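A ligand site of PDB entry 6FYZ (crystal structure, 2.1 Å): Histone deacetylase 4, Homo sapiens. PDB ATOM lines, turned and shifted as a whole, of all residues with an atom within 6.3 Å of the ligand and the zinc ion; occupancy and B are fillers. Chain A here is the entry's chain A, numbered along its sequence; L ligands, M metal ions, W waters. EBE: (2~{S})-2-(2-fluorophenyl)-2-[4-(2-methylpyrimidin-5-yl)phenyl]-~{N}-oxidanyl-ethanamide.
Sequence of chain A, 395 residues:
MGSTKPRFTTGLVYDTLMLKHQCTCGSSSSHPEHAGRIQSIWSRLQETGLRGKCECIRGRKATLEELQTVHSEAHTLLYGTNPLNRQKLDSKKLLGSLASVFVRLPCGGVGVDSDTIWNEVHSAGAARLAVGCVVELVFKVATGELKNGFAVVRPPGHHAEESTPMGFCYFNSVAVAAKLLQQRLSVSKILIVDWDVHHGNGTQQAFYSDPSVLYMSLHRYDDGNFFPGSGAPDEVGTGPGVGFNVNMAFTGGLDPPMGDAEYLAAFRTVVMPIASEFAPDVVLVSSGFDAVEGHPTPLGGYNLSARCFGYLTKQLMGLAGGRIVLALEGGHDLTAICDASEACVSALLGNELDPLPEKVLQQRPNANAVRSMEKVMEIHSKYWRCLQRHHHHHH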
ATOM      1  N   PRO A  32      16.712  -0.979  27.348  1.00  0.00           N
ATOM      2  CA  PRO A  32      16.804  -2.389  27.781  1.00  0.00           C
ATOM      3  C   PRO A  32      17.501  -2.659  29.135  1.00  0.00           C
ATOM      4  O   PRO A  32      17.312  -3.737  29.704  1.00  0.00           O
ATOM      5  CB  PRO A  32      17.558  -3.065  26.625  1.00  0.00           C
ATOM      6  CG  PRO A  32      18.278  -1.966  25.927  1.00  0.00           C
ATOM      7  CD  PRO A  32      17.445  -0.733  26.094  1.00  0.00           C
ATOM      8  N   GLU A  33      18.272  -1.698  29.637  1.00  0.00           N
ATOM      9  CA  GLU A  33      18.815  -1.796  30.990  1.00  0.00           C
ATOM     10  C   GLU A  33      17.838  -1.127  31.962  1.00  0.00           C
ATOM     11  O   GLU A  33      18.015   0.022  32.347  1.00  0.00           O
ATOM     12  CB  GLU A  33      20.226  -1.182  31.061  1.00  0.00           C
ATOM     13  CG  GLU A  33      21.081  -1.715  32.213  1.00  0.00           C
ATOM     14  CD  GLU A  33      20.502  -1.415  33.588  1.00  0.00           C
ATOM     15  OE1 GLU A  33      20.802  -0.305  34.115  1.00  0.00           O
ATOM     16  OE2 GLU A  33      19.754  -2.267  34.123  1.00  0.00           O
ATOM     17  N   HIS A  34      16.815  -1.881  32.389  1.00  0.00           N
ATOM     18  CA  HIS A  34      15.692  -1.354  33.178  1.00  0.00           C
ATOM     19  C   HIS A  34      15.499  -2.032  34.546  1.00  0.00           C
ATOM     20  O   HIS A  34      15.975  -3.158  34.769  1.00  0.00           O
ATOM     21  CB  HIS A  34      14.383  -1.433  32.367  1.00  0.00           C
ATOM     22  CG  HIS A  34      13.957  -2.823  32.035  1.00  0.00           C
ATOM     23  ND1 HIS A  34      13.046  -3.524  32.793  1.00  0.00           N
ATOM     24  CD2 HIS A  34      14.335  -3.659  31.035  1.00  0.00           C
ATOM     25  CE1 HIS A  34      12.884  -4.735  32.282  1.00  0.00           C
ATOM     26  NE2 HIS A  34      13.656  -4.831  31.215  1.00  0.00           N
ATOM     27  N   ARG A  37      14.777  -5.805  35.586  1.00  0.00           N
ATOM     28  CA  ARG A  37      15.819  -6.836  35.577  1.00  0.00           C
ATOM     29  C   ARG A  37      16.125  -7.340  36.991  1.00  0.00           C
ATOM     30  O   ARG A  37      16.087  -8.544  37.227  1.00  0.00           O
ATOM     31  CB  ARG A  37      17.098  -6.306  34.912  1.00  0.00           C
ATOM     32  CG  ARG A  37      16.959  -5.954  33.440  1.00  0.00           C
ATOM     33  CD  ARG A  37      18.208  -5.284  32.900  1.00  0.00           C
ATOM     34  NE  ARG A  37      19.341  -6.203  32.986  1.00  0.00           N
ATOM     35  CZ  ARG A  37      20.453  -6.027  33.691  1.00  0.00           C
ATOM     36  NH1 ARG A  37      21.382  -6.989  33.674  1.00  0.00           N
ATOM     37  NH2 ARG A  37      20.685  -4.917  34.394  1.00  0.00           N
ATOM     38  N   PRO A 156      24.877  -1.951  35.477  1.00  0.00           N
ATOM     39  CA  PRO A 156      26.068  -2.790  35.338  1.00  0.00           C
ATOM     40  C   PRO A 156      27.358  -1.956  35.320  1.00  0.00           C
ATOM     41  O   PRO A 156      27.305  -0.723  35.219  1.00  0.00           O
ATOM     42  CB  PRO A 156      25.844  -3.468  33.994  1.00  0.00           C
ATOM     43  CG  PRO A 156      25.054  -2.473  33.227  1.00  0.00           C
ATOM     44  CD  PRO A 156      24.144  -1.841  34.210  1.00  0.00           C
ATOM     45  N   HIS A 158      30.907  -3.301  33.936  1.00  0.00           N
ATOM     46  CA  HIS A 158      32.132  -3.778  33.293  1.00  0.00           C
ATOM     47  C   HIS A 158      32.613  -2.992  32.058  1.00  0.00           C
ATOM     48  O   HIS A 158      33.787  -3.082  31.706  1.00  0.00           O
ATOM     49  CB  HIS A 158      32.084  -5.300  33.078  1.00  0.00           C
ATOM     50  CG  HIS A 158      31.218  -5.779  31.951  1.00  0.00           C
ATOM     51  ND1 HIS A 158      31.479  -6.932  31.264  1.00  0.00           N
ATOM     52  CD2 HIS A 158      30.082  -5.253  31.402  1.00  0.00           C
ATOM     53  CE1 HIS A 158      30.559  -7.112  30.339  1.00  0.00           C
ATOM     54  NE2 HIS A 158      29.696  -6.107  30.400  1.00  0.00           N
ATOM     55  N   HIS A 159      31.731  -2.194  31.425  1.00  0.00           N
ATOM     56  CA  HIS A 159      32.155  -1.308  30.340  1.00  0.00           C
ATOM     57  C   HIS A 159      32.672   0.071  30.784  1.00  0.00           C
ATOM     58  O   HIS A 159      33.228   0.805  29.958  1.00  0.00           O
ATOM     59  CB  HIS A 159      31.024  -1.089  29.335  1.00  0.00           C
ATOM     60  CG  HIS A 159      30.563  -2.341  28.648  1.00  0.00           C
ATOM     61  ND1 HIS A 159      31.421  -3.169  27.962  1.00  0.00           N
ATOM     62  CD2 HIS A 159      29.334  -2.876  28.529  1.00  0.00           C
ATOM     63  CE1 HIS A 159      30.731  -4.178  27.454  1.00  0.00           C
ATOM     64  NE2 HIS A 159      29.457  -4.024  27.791  1.00  0.00           N
ATOM     65  N   MET A 166      30.104   3.808  29.349  1.00  0.00           N
ATOM     66  CA  MET A 166      29.551   3.242  28.099  1.00  0.00           C
ATOM     67  C   MET A 166      28.804   1.954  28.361  1.00  0.00           C
ATOM     68  O   MET A 166      28.890   1.390  29.448  1.00  0.00           O
ATOM     69  CB  MET A 166      30.630   3.018  27.017  1.00  0.00           C
ATOM     70  CG  MET A 166      31.872   2.284  27.483  1.00  0.00           C
ATOM     71  SD  MET A 166      32.832   1.598  26.099  1.00  0.00           S
ATOM     72  CE  MET A 166      31.824   0.206  25.615  1.00  0.00           C
ATOM     73  N   GLY A 167      28.028   1.539  27.371  1.00  0.00           N
ATOM     74  CA  GLY A 167      27.269   0.293  27.455  1.00  0.00           C
ATOM     75  C   GLY A 167      26.369   0.200  28.673  1.00  0.00           C
ATOM     76  O   GLY A 167      26.272  -0.850  29.295  1.00  0.00           O
ATOM     77  N   PHE A 168      25.714   1.318  28.994  1.00  0.00           N
ATOM     78  CA  PHE A 168      24.830   1.428  30.180  1.00  0.00           C
ATOM     79  C   PHE A 168      25.546   1.284  31.538  1.00  0.00           C
ATOM     80  O   PHE A 168      24.887   1.042  32.543  1.00  0.00           O
ATOM     81  CB  PHE A 168      23.640   0.457  30.094  1.00  0.00           C
ATOM     82  CG  PHE A 168      22.969   0.422  28.741  1.00  0.00           C
ATOM     83  CD1 PHE A 168      22.649   1.604  28.060  1.00  0.00           C
ATOM     84  CD2 PHE A 168      22.611  -0.801  28.166  1.00  0.00           C
ATOM     85  CE1 PHE A 168      22.019   1.557  26.819  1.00  0.00           C
ATOM     86  CE2 PHE A 168      21.967  -0.846  26.924  1.00  0.00           C
ATOM     87  CZ  PHE A 168      21.675   0.338  26.254  1.00  0.00           C
ATOM     88  N   CYS A 169      26.873   1.462  31.561  1.00  0.00           N
ATOM     89  CA  CYS A 169      27.685   1.393  32.779  1.00  0.00           C
ATOM     90  C   CYS A 169      28.290   2.762  33.077  1.00  0.00           C
ATOM     91  O   CYS A 169      28.666   3.497  32.156  1.00  0.00           O
ATOM     92  CB  CYS A 169      28.822   0.362  32.629  1.00  0.00           C
ATOM     93  SG  CYS A 169      28.346  -1.271  32.024  1.00  0.00           S
ATOM     94  N   ASP A 196      29.764 -12.481  31.106  1.00  0.00           N
ATOM     95  CA  ASP A 196      28.895 -11.677  30.269  1.00  0.00           C
ATOM     96  C   ASP A 196      29.357 -11.904  28.824  1.00  0.00           C
ATOM     97  O   ASP A 196      30.554 -12.072  28.554  1.00  0.00           O
ATOM     98  CB  ASP A 196      29.005 -10.209  30.669  1.00  0.00           C
ATOM     99  CG  ASP A 196      27.975  -9.348  29.996  1.00  0.00           C
ATOM    100  OD1 ASP A 196      28.122  -9.095  28.784  1.00  0.00           O
ATOM    101  OD2 ASP A 196      27.021  -8.901  30.694  1.00  0.00           O
ATOM    102  N   VAL A 197      28.410 -11.940  27.881  1.00  0.00           N
ATOM    103  CA  VAL A 197      28.733 -12.255  26.479  1.00  0.00           C
ATOM    104  C   VAL A 197      29.506 -11.131  25.765  1.00  0.00           C
ATOM    105  O   VAL A 197      30.098 -11.373  24.706  1.00  0.00           O
ATOM    106  CB  VAL A 197      27.454 -12.652  25.688  1.00  0.00           C
ATOM    107  CG1 VAL A 197      26.667 -11.429  25.239  1.00  0.00           C
ATOM    108  CG2 VAL A 197      27.804 -13.537  24.507  1.00  0.00           C
ATOM    109  N   HIS A 198      29.498  -9.930  26.342  1.00  0.00           N
ATOM    110  CA  HIS A 198      30.307  -8.812  25.831  1.00  0.00           C
ATOM    111  C   HIS A 198      31.604  -8.644  26.634  1.00  0.00           C
ATOM    112  O   HIS A 198      31.638  -8.954  27.823  1.00  0.00           O
ATOM    113  CB  HIS A 198      29.506  -7.503  25.858  1.00  0.00           C
ATOM    114  CG  HIS A 198      28.152  -7.626  25.238  1.00  0.00           C
ATOM    115  ND1 HIS A 198      27.021  -7.839  25.977  1.00  0.00           N
ATOM    116  CD2 HIS A 198      27.757  -7.564  23.943  1.00  0.00           C
ATOM    117  CE1 HIS A 198      25.974  -7.927  25.172  1.00  0.00           C
ATOM    118  NE2 HIS A 198      26.394  -7.738  23.930  1.00  0.00           N
ATOM    119  N   HIS A 199      32.651  -8.155  25.984  1.00  0.00           N
ATOM    120  CA  HIS A 199      33.943  -7.924  26.630  1.00  0.00           C
ATOM    121  C   HIS A 199      33.843  -6.786  27.656  1.00  0.00           C
ATOM    122  O   HIS A 199      33.325  -5.719  27.327  1.00  0.00           O
ATOM    123  CB  HIS A 199      34.989  -7.548  25.579  1.00  0.00           C
ATOM    124  CG  HIS A 199      36.366  -7.318  26.121  1.00  0.00           C
ATOM    125  ND1 HIS A 199      37.076  -6.157  25.901  1.00  0.00           N
ATOM    126  CD2 HIS A 199      37.178  -8.110  26.869  1.00  0.00           C
ATOM    127  CE1 HIS A 199      38.262  -6.242  26.484  1.00  0.00           C
ATOM    128  NE2 HIS A 199      38.338  -7.417  27.079  1.00  0.00           N
ATOM    129  N   PHE A 227      30.012  -6.134  19.744  1.00  0.00           N
ATOM    130  CA  PHE A 227      30.027  -5.075  20.736  1.00  0.00           C
ATOM    131  C   PHE A 227      30.805  -5.526  21.990  1.00  0.00           C
ATOM    132  O   PHE A 227      30.513  -6.596  22.507  1.00  0.00           O
ATOM    133  CB  PHE A 227      28.603  -4.678  21.135  1.00  0.00           C
ATOM    134  CG  PHE A 227      28.561  -3.598  22.173  1.00  0.00           C
ATOM    135  CD1 PHE A 227      28.613  -2.270  21.802  1.00  0.00           C
ATOM    136  CD2 PHE A 227      28.518  -3.924  23.524  1.00  0.00           C
ATOM    137  CE1 PHE A 227      28.603  -1.270  22.760  1.00  0.00           C
ATOM    138  CE2 PHE A 227      28.501  -2.934  24.477  1.00  0.00           C
ATOM    139  CZ  PHE A 227      28.553  -1.606  24.106  1.00  0.00           C
ATOM    140  N   GLY A 288      27.180 -11.452  33.802  1.00  0.00           N
ATOM    141  CA  GLY A 288      26.110 -11.156  32.854  1.00  0.00           C
ATOM    142  C   GLY A 288      25.475 -12.457  32.374  1.00  0.00           C
ATOM    143  O   GLY A 288      26.159 -13.455  32.226  1.00  0.00           O
ATOM    144  N   ASP A 290      23.589 -12.691  29.438  1.00  0.00           N
ATOM    145  CA  ASP A 290      23.158 -12.417  28.059  1.00  0.00           C
ATOM    146  C   ASP A 290      23.701 -13.411  27.016  1.00  0.00           C
ATOM    147  O   ASP A 290      23.322 -13.330  25.850  1.00  0.00           O
ATOM    148  CB  ASP A 290      23.419 -10.944  27.658  1.00  0.00           C
ATOM    149  CG  ASP A 290      24.806 -10.443  28.045  1.00  0.00           C
ATOM    150  OD1 ASP A 290      25.676 -11.255  28.406  1.00  0.00           O
ATOM    151  OD2 ASP A 290      25.021  -9.214  27.970  1.00  0.00           O
ATOM    152  N   PRO A 298      22.265  -7.484  18.798  1.00  0.00           N
ATOM    153  CA  PRO A 298      23.601  -7.550  19.405  1.00  0.00           C
ATOM    154  C   PRO A 298      23.650  -7.630  20.946  1.00  0.00           C
ATOM    155  O   PRO A 298      24.719  -7.390  21.528  1.00  0.00           O
ATOM    156  CB  PRO A 298      24.214  -6.235  18.926  1.00  0.00           C
ATOM    157  CG  PRO A 298      23.070  -5.282  18.960  1.00  0.00           C
ATOM    158  CD  PRO A 298      21.816  -6.089  18.679  1.00  0.00           C
ATOM    159  N   LEU A 299      22.536  -7.943  21.594  1.00  0.00           N
ATOM    160  CA  LEU A 299      22.511  -8.178  23.042  1.00  0.00           C
ATOM    161  C   LEU A 299      23.068  -9.552  23.396  1.00  0.00           C
ATOM    162  O   LEU A 299      23.462  -9.784  24.537  1.00  0.00           O
ATOM    163  CB  LEU A 299      21.100  -8.043  23.602  1.00  0.00           C
ATOM    164  CG  LEU A 299      20.415  -6.686  23.435  1.00  0.00           C
ATOM    165  CD1 LEU A 299      18.943  -6.793  23.791  1.00  0.00           C
ATOM    166  CD2 LEU A 299      21.111  -5.624  24.262  1.00  0.00           C
ATOM    167  N   GLU A 329      25.855  -8.320  35.653  1.00  0.00           N
ATOM    168  CA  GLU A 329      26.280  -7.358  34.663  1.00  0.00           C
ATOM    169  C   GLU A 329      25.124  -7.253  33.656  1.00  0.00           C
ATOM    170  O   GLU A 329      24.075  -6.699  34.017  1.00  0.00           O
ATOM    171  CB  GLU A 329      27.620  -7.749  34.037  1.00  0.00           C
ATOM    172  CG  GLU A 329      28.802  -7.756  35.018  1.00  0.00           C
ATOM    173  CD  GLU A 329      29.355  -6.374  35.366  1.00  0.00           C
ATOM    174  OE1 GLU A 329      28.820  -5.343  34.907  1.00  0.00           O
ATOM    175  OE2 GLU A 329      30.344  -6.324  36.124  1.00  0.00           O
ATOM    176  N   GLY A 330      25.284  -7.780  32.443  1.00  0.00           N
ATOM    177  CA  GLY A 330      24.233  -7.766  31.422  1.00  0.00           C
ATOM    178  C   GLY A 330      23.227  -8.887  31.570  1.00  0.00           C
ATOM    179  O   GLY A 330      23.148  -9.554  32.614  1.00  0.00           O
ATOM    180  N   GLY A 331      22.440  -9.094  30.521  1.00  0.00           N
ATOM    181  CA  GLY A 331      21.302 -10.016  30.582  1.00  0.00           C
ATOM    182  C   GLY A 331      20.041  -9.196  30.673  1.00  0.00           C
ATOM    183  O   GLY A 331      19.856  -8.397  31.590  1.00  0.00           O
ATOM    184  N   HIS A 332      19.152  -9.446  29.710  1.00  0.00           N
ATOM    185  CA  HIS A 332      18.006  -8.597  29.385  1.00  0.00           C
ATOM    186  C   HIS A 332      16.680  -9.366  29.515  1.00  0.00           C
ATOM    187  O   HIS A 332      15.743  -8.902  30.190  1.00  0.00           O
ATOM    188  CB  HIS A 332      18.207  -8.079  27.963  1.00  0.00           C
ATOM    189  CG  HIS A 332      17.001  -7.438  27.366  1.00  0.00           C
ATOM    190  ND1 HIS A 332      16.621  -6.154  27.667  1.00  0.00           N
ATOM    191  CD2 HIS A 332      16.099  -7.907  26.479  1.00  0.00           C
ATOM    192  CE1 HIS A 332      15.518  -5.862  27.004  1.00  0.00           C
ATOM    193  NE2 HIS A 332      15.189  -6.903  26.270  1.00  0.00           N
HETATM  194  C4  EBE L   1      25.105  -2.394  26.286  1.00  0.00           C
HETATM  195  C5  EBE L   1      25.162  -1.984  24.954  1.00  0.00           C
HETATM  196  C6  EBE L   1      25.017  -2.892  23.892  1.00  0.00           C
HETATM  197  C7  EBE L   1      25.078  -2.446  22.443  1.00  0.00           C
HETATM  198  C8  EBE L   1      25.076  -1.084  22.087  1.00  0.00           C
HETATM  199  C3  EBE L   1      24.906  -3.722  26.610  1.00  0.00           C
HETATM  200  C2  EBE L   1      24.752  -4.637  25.576  1.00  0.00           C
HETATM  201  C10 EBE L   1      25.169  -1.619  19.798  1.00  0.00           C
HETATM  202  C1  EBE L   1      24.815  -4.239  24.239  1.00  0.00           C
HETATM  203  C19 EBE L   1      22.305  -4.347  27.741  1.00  0.00           C
HETATM  204  C12 EBE L   1      25.125  -3.361  21.374  1.00  0.00           C
HETATM  205  C13 EBE L   1      24.837  -4.121  28.053  1.00  0.00           C
HETATM  206  C14 EBE L   1      23.444  -4.333  28.556  1.00  0.00           C
HETATM  207  C18 EBE L   1      21.045  -4.563  28.282  1.00  0.00           C
HETATM  208  N9  EBE L   1      25.134  -0.712  20.789  1.00  0.00           N
HETATM  209  C20 EBE L   1      25.648  -5.384  28.280  1.00  0.00           C
HETATM  210  C24 EBE L   1      25.236  -1.174  18.362  1.00  0.00           C
HETATM  211  O21 EBE L   1      25.106  -6.479  28.331  1.00  0.00           O
HETATM  212  N22 EBE L   1      26.961  -5.250  28.446  1.00  0.00           N
HETATM  213  O23 EBE L   1      27.759  -6.371  28.656  1.00  0.00           O
HETATM  214  C17 EBE L   1      20.894  -4.757  29.646  1.00  0.00           C
HETATM  215  C16 EBE L   1      22.017  -4.758  30.459  1.00  0.00           C
HETATM  216  C15 EBE L   1      23.277  -4.537  29.926  1.00  0.00           C
HETATM  217  F25 EBE L   1      24.340  -4.551  30.759  1.00  0.00           F
HETATM  218  N11 EBE L   1      25.172  -2.937  20.104  1.00  0.00           N
HETATM  219 ZN    ZN M   1      26.659  -8.005  28.016  1.00  0.00          ZN
HETATM  220  O   HOH W   1      22.463  -7.655  28.027  1.00  0.00           O
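NE2 of His 158 sits at hydrogen-bond distance from N22 of the ligand (3.5 Å). N22 of the ligand sits at hydrogen-bond distance from NE2 of His 159, at 2.9 Å.
The backbone carbonyl oxygen (O) of Pro 298 lies within hydrogen-bond range of a ring nitrogen (NE2) of His 198 (2.9 Å). NE2 of His 158 sits at hydrogen-bond distance from NE2 of His 159 (3.3 Å). N of His 158 sits at hydrogen-bond distance from OE1 of Glu 329, 3.1 Å away. The backbone NH (N) of His 158 sits at hydrogen-bond distance from the side-chain sulfur (SG) of Cys 169 (3.8 Å). The backbone NH (N) of His 159 lies within hydrogen-bond range of the side-chain sulfur (SG) of Cys 169. The guanidinium group of Arg 37 is in hydrogen-bond range of the backbone carbonyl oxygen of Gly 330, at 3.3 Å. The backbone carbonyl oxygen (O) of Pro 156 lies close to the side-chain sulfur (SG) of Cys 169 (3.4 Å). The backbone carbonyl oxygen of Gly 167 lies within hydrogen-bond range of the side-chain sulfur of Cys 169 (3.5 Å).
Pro 32 touches the ligand. Glu 33 touches the ligand (CG to C16, 3.6 Å). Arg 37 touches the ligand (CZ to C16, 3.8 Å). CG of Pro 156 touches F25 of the ligand, 3.3 Å away. Gly 167 touches the ligand. Phe 168 touches the ligand (CD2 to C4, 3.5 Å). Phe 227 touches the ligand. Pro 298 touches the ligand. Leu 299 touches the ligand. O of Glu 329 touches F25 of the ligand (3.9 Å). Gly 330 touches the ligand. Hydrophobic or aromatic side chains within 4 Å of the ligand: Pro 156, His 158, His 159, Phe 168, His 198, Phe 227, Pro 298 and Leu 299. Of the 24 residues printed, 16 come within 4 Å of the ligand. Along chain A the residues within 4 Å of the ligand span positions 32 to 330. The nearest printed residue that does not touch the ligand is Gly 331 (4.3 Å).
Three residues have an atom within 4 Å of the zinc ion: Asp 196, His 198 and Asp 290.
OD1 of Asp 196 binds the zinc ion, at 2.0 Å. The zinc ion is bound by OD2 of Asp 290, at 2.0 Å. The zinc ion is bound by O23 of the ligand, 2.1 Å away. A ring nitrogen (ND1) of His 198 is bound to the zinc ion, 2.1 Å away. The zinc ion is bound by an oxygen (O21) of the ligand. Slightly farther from the zinc ion lies the side-chain carboxylate (OD2) of Asp 196 (2.8 Å).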
